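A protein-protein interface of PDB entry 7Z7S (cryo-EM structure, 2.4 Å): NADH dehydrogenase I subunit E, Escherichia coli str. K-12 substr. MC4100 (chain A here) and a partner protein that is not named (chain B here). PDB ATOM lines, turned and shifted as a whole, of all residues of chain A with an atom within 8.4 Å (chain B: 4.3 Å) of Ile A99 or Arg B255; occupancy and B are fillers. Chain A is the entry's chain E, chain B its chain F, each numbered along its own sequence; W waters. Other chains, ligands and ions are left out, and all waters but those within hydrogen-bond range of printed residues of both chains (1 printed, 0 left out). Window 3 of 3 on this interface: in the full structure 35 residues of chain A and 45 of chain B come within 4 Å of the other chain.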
ATOM      1  N   ASP A  93     -36.739  -8.990 -25.951  1.00  0.00           N
ATOM      2  CA  ASP A  93     -35.724  -8.250 -25.214  1.00  0.00           C
ATOM      3  C   ASP A  93     -35.876  -8.430 -23.707  1.00  0.00           C
ATOM      4  O   ASP A  93     -35.447  -7.579 -22.930  1.00  0.00           O
ATOM      5  CB  ASP A  93     -35.733  -6.767 -25.600  1.00  0.00           C
ATOM      6  CG  ASP A  93     -37.011  -6.035 -25.211  1.00  0.00           C
ATOM      7  OD1 ASP A  93     -38.012  -6.663 -24.826  1.00  0.00           O
ATOM      8  OD2 ASP A  93     -37.008  -4.794 -25.303  1.00  0.00           O
ATOM      9  N   SER A  94     -36.474  -9.534 -23.281  1.00  0.00           N
ATOM     10  CA  SER A  94     -36.738  -9.770 -21.872  1.00  0.00           C
ATOM     11  C   SER A  94     -35.536 -10.453 -21.218  1.00  0.00           C
ATOM     12  O   SER A  94     -34.492 -10.642 -21.840  1.00  0.00           O
ATOM     13  CB  SER A  94     -38.025 -10.566 -21.709  1.00  0.00           C
ATOM     14  OG  SER A  94     -39.149  -9.738 -21.918  1.00  0.00           O
ATOM     15  N   VAL A  95     -35.694 -10.851 -19.953  1.00  0.00           N
ATOM     16  CA  VAL A  95     -34.545 -11.055 -19.071  1.00  0.00           C
ATOM     17  C   VAL A  95     -33.765 -12.318 -19.434  1.00  0.00           C
ATOM     18  O   VAL A  95     -32.529 -12.309 -19.434  1.00  0.00           O
ATOM     19  CB  VAL A  95     -35.001 -11.044 -17.596  1.00  0.00           C
ATOM     20  CG1 VAL A  95     -36.110 -12.043 -17.327  1.00  0.00           C
ATOM     21  CG2 VAL A  95     -33.836 -11.265 -16.663  1.00  0.00           C
ATOM     22  N   VAL A  96     -34.455 -13.414 -19.756  1.00  0.00           N
ATOM     23  CA  VAL A  96     -33.748 -14.656 -20.062  1.00  0.00           C
ATOM     24  C   VAL A  96     -33.036 -14.550 -21.402  1.00  0.00           C
ATOM     25  O   VAL A  96     -31.906 -15.025 -21.556  1.00  0.00           O
ATOM     26  CB  VAL A  96     -34.707 -15.858 -20.024  1.00  0.00           C
ATOM     27  CG1 VAL A  96     -33.919 -17.147 -19.964  1.00  0.00           C
ATOM     28  CG2 VAL A  96     -35.641 -15.754 -18.841  1.00  0.00           C
ATOM     29  N   CYS A  97     -33.674 -13.923 -22.390  1.00  0.00           N
ATOM     30  CA  CYS A  97     -33.009 -13.712 -23.668  1.00  0.00           C
ATOM     31  C   CYS A  97     -31.895 -12.681 -23.554  1.00  0.00           C
ATOM     32  O   CYS A  97     -30.950 -12.706 -24.344  1.00  0.00           O
ATOM     33  CB  CYS A  97     -34.024 -13.297 -24.727  1.00  0.00           C
ATOM     34  SG  CYS A  97     -35.167 -14.601 -25.183  1.00  0.00           S
ATOM     35  N   HIS A  98     -31.994 -11.771 -22.586  1.00  0.00           N
ATOM     36  CA  HIS A  98     -30.880 -10.882 -22.280  1.00  0.00           C
ATOM     37  C   HIS A  98     -29.704 -11.660 -21.708  1.00  0.00           C
ATOM     38  O   HIS A  98     -28.549 -11.395 -22.053  1.00  0.00           O
ATOM     39  CB  HIS A  98     -31.343  -9.793 -21.313  1.00  0.00           C
ATOM     40  CG  HIS A  98     -30.244  -8.913 -20.812  1.00  0.00           C
ATOM     41  ND1 HIS A  98     -29.568  -9.161 -19.639  1.00  0.00           N
ATOM     42  CD2 HIS A  98     -29.713  -7.776 -21.318  1.00  0.00           C
ATOM     43  CE1 HIS A  98     -28.663  -8.221 -19.447  1.00  0.00           C
ATOM     44  NE2 HIS A  98     -28.733  -7.366 -20.451  1.00  0.00           N
ATOM     45  N   ILE A  99     -29.986 -12.621 -20.831  1.00  0.00           N
ATOM     46  CA  ILE A  99     -28.952 -13.512 -20.320  1.00  0.00           C
ATOM     47  C   ILE A  99     -28.385 -14.367 -21.447  1.00  0.00           C
ATOM     48  O   ILE A  99     -27.174 -14.591 -21.531  1.00  0.00           O
ATOM     49  CB  ILE A  99     -29.527 -14.363 -19.172  1.00  0.00           C
ATOM     50  CG1 ILE A  99     -29.736 -13.494 -17.937  1.00  0.00           C
ATOM     51  CG2 ILE A  99     -28.634 -15.528 -18.839  1.00  0.00           C
ATOM     52  CD1 ILE A  99     -30.215 -14.246 -16.728  1.00  0.00           C
ATOM     53  N   ASN A 100     -29.246 -14.824 -22.351  1.00  0.00           N
ATOM     54  CA  ASN A 100     -28.827 -15.631 -23.488  1.00  0.00           C
ATOM     55  C   ASN A 100     -28.272 -14.803 -24.638  1.00  0.00           C
ATOM     56  O   ASN A 100     -27.874 -15.377 -25.654  1.00  0.00           O
ATOM     57  CB  ASN A 100     -29.994 -16.482 -23.978  1.00  0.00           C
ATOM     58  CG  ASN A 100     -30.296 -17.625 -23.047  1.00  0.00           C
ATOM     59  OD1 ASN A 100     -29.390 -18.266 -22.529  1.00  0.00           O
ATOM     60  ND2 ASN A 100     -31.574 -17.880 -22.818  1.00  0.00           N
ATOM     61  N   GLY A 101     -28.247 -13.482 -24.513  1.00  0.00           N
ATOM     62  CA  GLY A 101     -27.575 -12.649 -25.487  1.00  0.00           C
ATOM     63  C   GLY A 101     -28.423 -12.194 -26.652  1.00  0.00           C
ATOM     64  O   GLY A 101     -28.036 -12.381 -27.807  1.00  0.00           O
ATOM     65  N   TYR A 102     -29.572 -11.576 -26.371  1.00  0.00           N
ATOM     66  CA  TYR A 102     -30.363 -10.988 -27.442  1.00  0.00           C
ATOM     67  C   TYR A 102     -29.697  -9.763 -28.046  1.00  0.00           C
ATOM     68  O   TYR A 102     -30.103  -9.341 -29.129  1.00  0.00           O
ATOM     69  CB  TYR A 102     -31.773 -10.621 -26.950  1.00  0.00           C
ATOM     70  CG  TYR A 102     -31.925  -9.209 -26.407  1.00  0.00           C
ATOM     71  CD1 TYR A 102     -31.664  -8.936 -25.080  1.00  0.00           C
ATOM     72  CD2 TYR A 102     -32.341  -8.154 -27.216  1.00  0.00           C
ATOM     73  CE1 TYR A 102     -31.790  -7.669 -24.571  1.00  0.00           C
ATOM     74  CE2 TYR A 102     -32.444  -6.883 -26.720  1.00  0.00           C
ATOM     75  CZ  TYR A 102     -32.181  -6.648 -25.392  1.00  0.00           C
ATOM     76  OH  TYR A 102     -32.305  -5.383 -24.876  1.00  0.00           O
ATOM     77  N   GLN A 103     -28.732  -9.153 -27.353  1.00  0.00           N
ATOM     78  CA  GLN A 103     -28.124  -7.924 -27.854  1.00  0.00           C
ATOM     79  C   GLN A 103     -27.344  -8.169 -29.137  1.00  0.00           C
ATOM     80  O   GLN A 103     -27.358  -7.330 -30.042  1.00  0.00           O
ATOM     81  CB  GLN A 103     -27.221  -7.308 -26.792  1.00  0.00           C
ATOM     82  CG  GLN A 103     -27.929  -6.335 -25.883  1.00  0.00           C
ATOM     83  CD  GLN A 103     -28.000  -6.832 -24.464  1.00  0.00           C
ATOM     84  OE1 GLN A 103     -28.102  -8.031 -24.223  1.00  0.00           O
ATOM     85  NE2 GLN A 103     -27.935  -5.912 -23.512  1.00  0.00           N
ATOM     86  N   CYS A 137     -38.333 -19.238 -23.206  1.00  0.00           N
ATOM     87  CA  CYS A 137     -37.093 -18.793 -22.588  1.00  0.00           C
ATOM     88  C   CYS A 137     -36.060 -19.899 -22.454  1.00  0.00           C
ATOM     89  O   CYS A 137     -34.867 -19.599 -22.366  1.00  0.00           O
ATOM     90  CB  CYS A 137     -37.397 -18.185 -21.225  1.00  0.00           C
ATOM     91  SG  CYS A 137     -38.981 -17.364 -21.177  1.00  0.00           S
ATOM     92  N   ASP A 138     -36.476 -21.163 -22.446  1.00  0.00           N
ATOM     93  CA  ASP A 138     -35.506 -22.248 -22.410  1.00  0.00           C
ATOM     94  C   ASP A 138     -34.782 -22.432 -23.736  1.00  0.00           C
ATOM     95  O   ASP A 138     -33.758 -23.120 -23.770  1.00  0.00           O
ATOM     96  CB  ASP A 138     -36.183 -23.557 -22.006  1.00  0.00           C
ATOM     97  CG  ASP A 138     -37.487 -23.785 -22.731  1.00  0.00           C
ATOM     98  OD1 ASP A 138     -37.946 -22.873 -23.443  1.00  0.00           O
ATOM     99  OD2 ASP A 138     -38.058 -24.882 -22.591  1.00  0.00           O
ATOM    100  N   GLY A 140     -33.881 -19.696 -25.813  1.00  0.00           N
ATOM    101  CA  GLY A 140     -33.534 -18.358 -26.219  1.00  0.00           C
ATOM    102  C   GLY A 140     -32.152 -18.241 -26.828  1.00  0.00           C
ATOM    103  O   GLY A 140     -31.337 -19.162 -26.746  1.00  0.00           O
ATOM    104  N   PRO A 141     -31.854 -17.092 -27.457  1.00  0.00           N
ATOM    105  CA  PRO A 141     -32.747 -15.950 -27.678  1.00  0.00           C
ATOM    106  C   PRO A 141     -33.753 -16.185 -28.800  1.00  0.00           C
ATOM    107  O   PRO A 141     -33.455 -16.877 -29.762  1.00  0.00           O
ATOM    108  CB  PRO A 141     -31.781 -14.823 -28.034  1.00  0.00           C
ATOM    109  CG  PRO A 141     -30.618 -15.497 -28.601  1.00  0.00           C
ATOM    110  CD  PRO A 141     -30.485 -16.805 -27.910  1.00  0.00           C
ATOM    111  N   GLY B 254     -31.531 -20.365 -18.566  1.00  0.00           N
ATOM    112  CA  GLY B 254     -30.503 -19.350 -18.659  1.00  0.00           C
ATOM    113  C   GLY B 254     -29.096 -19.859 -18.441  1.00  0.00           C
ATOM    114  O   GLY B 254     -28.637 -19.961 -17.301  1.00  0.00           O
ATOM    115  N   ARG B 255     -28.401 -20.149 -19.545  1.00  0.00           N
ATOM    116  CA  ARG B 255     -26.988 -20.544 -19.565  1.00  0.00           C
ATOM    117  C   ARG B 255     -26.697 -21.755 -18.686  1.00  0.00           C
ATOM    118  O   ARG B 255     -25.598 -21.895 -18.151  1.00  0.00           O
ATOM    119  CB  ARG B 255     -26.079 -19.374 -19.189  1.00  0.00           C
ATOM    120  CG  ARG B 255     -26.391 -18.120 -19.966  1.00  0.00           C
ATOM    121  CD  ARG B 255     -25.227 -17.626 -20.788  1.00  0.00           C
ATOM    122  NE  ARG B 255     -24.519 -16.552 -20.105  1.00  0.00           N
ATOM    123  CZ  ARG B 255     -23.368 -16.036 -20.509  1.00  0.00           C
ATOM    124  NH1 ARG B 255     -22.770 -16.459 -21.610  1.00  0.00           N
ATOM    125  NH2 ARG B 255     -22.803 -15.071 -19.792  1.00  0.00           N
ATOM    126  N   VAL B 256     -27.667 -22.646 -18.543  1.00  0.00           N
ATOM    127  CA  VAL B 256     -27.447 -23.926 -17.919  1.00  0.00           C
ATOM    128  C   VAL B 256     -27.230 -24.950 -19.025  1.00  0.00           C
ATOM    129  O   VAL B 256     -27.461 -24.682 -20.200  1.00  0.00           O
ATOM    130  CB  VAL B 256     -28.610 -24.324 -16.987  1.00  0.00           C
ATOM    131  CG1 VAL B 256     -28.551 -23.524 -15.713  1.00  0.00           C
ATOM    132  CG2 VAL B 256     -29.931 -24.112 -17.673  1.00  0.00           C
ATOM    133  N   MET B 281     -24.618 -25.354 -14.288  1.00  0.00           N
ATOM    134  CA  MET B 281     -24.251 -24.226 -15.122  1.00  0.00           C
ATOM    135  C   MET B 281     -23.411 -24.704 -16.301  1.00  0.00           C
ATOM    136  O   MET B 281     -22.825 -25.789 -16.280  1.00  0.00           O
ATOM    137  CB  MET B 281     -23.483 -23.188 -14.301  1.00  0.00           C
ATOM    138  CG  MET B 281     -24.317 -22.510 -13.215  1.00  0.00           C
ATOM    139  SD  MET B 281     -25.416 -21.140 -13.644  1.00  0.00           S
ATOM    140  CE  MET B 281     -24.851 -20.652 -15.262  1.00  0.00           C
ATOM    141  N   ARG B 282     -23.363 -23.884 -17.347  1.00  0.00           N
ATOM    142  CA  ARG B 282     -22.583 -24.237 -18.521  1.00  0.00           C
ATOM    143  C   ARG B 282     -21.090 -24.124 -18.218  1.00  0.00           C
ATOM    144  O   ARG B 282     -20.674 -23.584 -17.189  1.00  0.00           O
ATOM    145  CB  ARG B 282     -22.965 -23.354 -19.707  1.00  0.00           C
ATOM    146  CG  ARG B 282     -23.655 -24.114 -20.820  1.00  0.00           C
ATOM    147  CD  ARG B 282     -24.491 -23.208 -21.699  1.00  0.00           C
ATOM    148  NE  ARG B 282     -23.775 -22.001 -22.088  1.00  0.00           N
ATOM    149  CZ  ARG B 282     -24.320 -20.994 -22.756  1.00  0.00           C
ATOM    150  NH1 ARG B 282     -25.587 -21.018 -23.129  1.00  0.00           N
ATOM    151  NH2 ARG B 282     -23.573 -19.937 -23.058  1.00  0.00           N
ATOM    152  N   LEU B 285     -18.778 -21.055 -16.636  1.00  0.00           N
ATOM    153  CA  LEU B 285     -19.674 -20.098 -16.003  1.00  0.00           C
ATOM    154  C   LEU B 285     -19.891 -20.501 -14.555  1.00  0.00           C
ATOM    155  O   LEU B 285     -20.144 -21.674 -14.264  1.00  0.00           O
ATOM    156  CB  LEU B 285     -21.012 -20.024 -16.740  1.00  0.00           C
ATOM    157  CG  LEU B 285     -20.967 -19.453 -18.156  1.00  0.00           C
ATOM    158  CD1 LEU B 285     -22.356 -19.394 -18.744  1.00  0.00           C
ATOM    159  CD2 LEU B 285     -20.331 -18.081 -18.154  1.00  0.00           C
ATOM    160  N   MET B 327     -34.667 -19.037 -12.980  1.00  0.00           N
ATOM    161  CA  MET B 327     -33.718 -18.523 -13.949  1.00  0.00           C
ATOM    162  C   MET B 327     -32.381 -18.339 -13.256  1.00  0.00           C
ATOM    163  O   MET B 327     -32.315 -17.729 -12.187  1.00  0.00           O
ATOM    164  CB  MET B 327     -34.212 -17.202 -14.547  1.00  0.00           C
ATOM    165  CG  MET B 327     -33.260 -16.546 -15.513  1.00  0.00           C
ATOM    166  SD  MET B 327     -33.716 -14.834 -15.805  1.00  0.00           S
ATOM    167  CE  MET B 327     -33.188 -14.084 -14.272  1.00  0.00           C
ATOM    168  N   ALA B 328     -31.327 -18.872 -13.861  1.00  0.00           N
ATOM    169  CA  ALA B 328     -29.988 -18.787 -13.302  1.00  0.00           C
ATOM    170  C   ALA B 328     -29.250 -17.584 -13.870  1.00  0.00           C
ATOM    171  O   ALA B 328     -29.349 -17.282 -15.060  1.00  0.00           O
ATOM    172  CB  ALA B 328     -29.201 -20.063 -13.594  1.00  0.00           C
ATOM    173  N   VAL B 329     -28.515 -16.898 -13.004  1.00  0.00           N
ATOM    174  CA  VAL B 329     -27.676 -15.768 -13.368  1.00  0.00           C
ATOM    175  C   VAL B 329     -26.239 -16.174 -13.090  1.00  0.00           C
ATOM    176  O   VAL B 329     -25.895 -16.488 -11.944  1.00  0.00           O
ATOM    177  CB  VAL B 329     -28.046 -14.507 -12.574  1.00  0.00           C
ATOM    178  CG1 VAL B 329     -27.286 -13.317 -13.097  1.00  0.00           C
ATOM    179  CG2 VAL B 329     -29.543 -14.261 -12.622  1.00  0.00           C
ATOM    180  N   ASP B 330     -25.407 -16.156 -14.129  1.00  0.00           N
ATOM    181  CA  ASP B 330     -24.006 -16.519 -14.014  1.00  0.00           C
ATOM    182  C   ASP B 330     -23.171 -15.297 -13.642  1.00  0.00           C
ATOM    183  O   ASP B 330     -23.671 -14.176 -13.537  1.00  0.00           O
ATOM    184  CB  ASP B 330     -23.502 -17.137 -15.315  1.00  0.00           C
ATOM    185  CG  ASP B 330     -23.808 -16.282 -16.520  1.00  0.00           C
ATOM    186  OD1 ASP B 330     -24.997 -16.004 -16.765  1.00  0.00           O
ATOM    187  OD2 ASP B 330     -22.860 -15.881 -17.222  1.00  0.00           O
ATOM    188  N   GLU B 332     -20.920 -13.733 -15.338  1.00  0.00           N
ATOM    189  CA  GLU B 332     -20.656 -12.795 -16.420  1.00  0.00           C
ATOM    190  C   GLU B 332     -21.753 -11.756 -16.591  1.00  0.00           C
ATOM    191  O   GLU B 332     -21.592 -10.840 -17.402  1.00  0.00           O
ATOM    192  CB  GLU B 332     -20.475 -13.547 -17.738  1.00  0.00           C
ATOM    193  CG  GLU B 332     -19.104 -14.153 -17.927  1.00  0.00           C
ATOM    194  CD  GLU B 332     -18.976 -14.876 -19.249  1.00  0.00           C
ATOM    195  OE1 GLU B 332     -19.757 -14.566 -20.171  1.00  0.00           O
ATOM    196  OE2 GLU B 332     -18.100 -15.755 -19.369  1.00  0.00           O
ATOM    197  N   ILE B 333     -22.854 -11.875 -15.863  1.00  0.00           N
ATOM    198  CA  ILE B 333     -23.998 -10.988 -16.015  1.00  0.00           C
ATOM    199  C   ILE B 333     -23.884  -9.876 -14.985  1.00  0.00           C
ATOM    200  O   ILE B 333     -23.826 -10.139 -13.780  1.00  0.00           O
ATOM    201  CB  ILE B 333     -25.320 -11.754 -15.863  1.00  0.00           C
ATOM    202  CG1 ILE B 333     -25.524 -12.699 -17.047  1.00  0.00           C
ATOM    203  CG2 ILE B 333     -26.484 -10.796 -15.737  1.00  0.00           C
ATOM    204  CD1 ILE B 333     -25.607 -11.996 -18.378  1.00  0.00           C
ATOM    205  N   LEU B 338     -29.015  -6.360 -15.686  1.00  0.00           N
ATOM    206  CA  LEU B 338     -30.132  -7.291 -15.586  1.00  0.00           C
ATOM    207  C   LEU B 338     -31.360  -6.626 -14.977  1.00  0.00           C
ATOM    208  O   LEU B 338     -32.480  -6.771 -15.482  1.00  0.00           O
ATOM    209  CB  LEU B 338     -29.718  -8.499 -14.755  1.00  0.00           C
ATOM    210  CG  LEU B 338     -30.565  -9.740 -14.962  1.00  0.00           C
ATOM    211  CD1 LEU B 338     -30.296 -10.280 -16.335  1.00  0.00           C
ATOM    212  CD2 LEU B 338     -30.240 -10.762 -13.907  1.00  0.00           C
HETATM  213  O   HOH W   1     -32.448 -20.418 -21.546  1.00  0.00           O
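The guanidinium group (NH2) of Arg B255 is in salt-bridge range of the side-chain carboxylate (OD2) of Asp B330, at 2.7 Å.
The backbone NH (N) of Arg B282 lies within hydrogen-bond range of the backbone carbonyl oxygen (O) of Arg B255, at 3.1 Å.
A ring nitrogen (NE2) of His A98 lies close to the side-chain amide nitrogen (NE2) of Gln A103 (3.5 Å).
The side-chain carboxylate of Glu B332 is in salt-bridge range of the guanidinium group of Arg B255 (3.1 Å).
ND2 of Asn A100 is in hydrogen-bond range of O of Val A96 (3.1 Å).
Among the printed residues, merely in contact across the chains: His A98 with Leu B338 (3.6 Å), Ile A99 with Ala B328 (3.6 Å), Ile A99 with Arg B255 (3.6 Å), Ile A99 with Leu B338 (3.6 Å), Asn A100 with Arg B255 (3.7 Å), Ile A99 with Met B327 (3.7 Å), Val A95 with Met B327 (3.7 Å), Val A95 with Leu B338 (3.7 Å) and Val A96 with Met B327 (3.7 Å).
Of the printed residues of chain B, Val A95 touches Met B327 and Leu B338.
Printed residues of chain B within 4 Å of His A98: Leu B338 (3.6 Å).
Ile A99 touches just these residues of chain B: Arg B255, Met B327, Ala B328 and Leu B338.
No residue of chain A comes within 4 Å of Gly B254.
Of chain A, only Ile A99 (3.6 Å) and Asn A100 (3.7 Å) come within 4 Å of Arg B255.
No residue of chain A comes within 4 Å of Val B256.
Val B329 touches none of the printed residues of chain A.
The nearest printed residue of chain B that does not touch Ile A99 is Ile B333 (4.2 Å).
Hydrophobic or aromatic side chains of chain A that line the printed part of chain B: Val A95, Val A96, His A98 and Ile A99.
Hydrophobic or aromatic side chains of chain B that line the printed part of chain A: Met B327 and Leu B338.
Water W1 lies within hydrogen-bond range of O of Cys A137 (2.7 Å), ND2 of Asn A100 (3.0 Å) and N of Gly B254 (3.1 Å).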
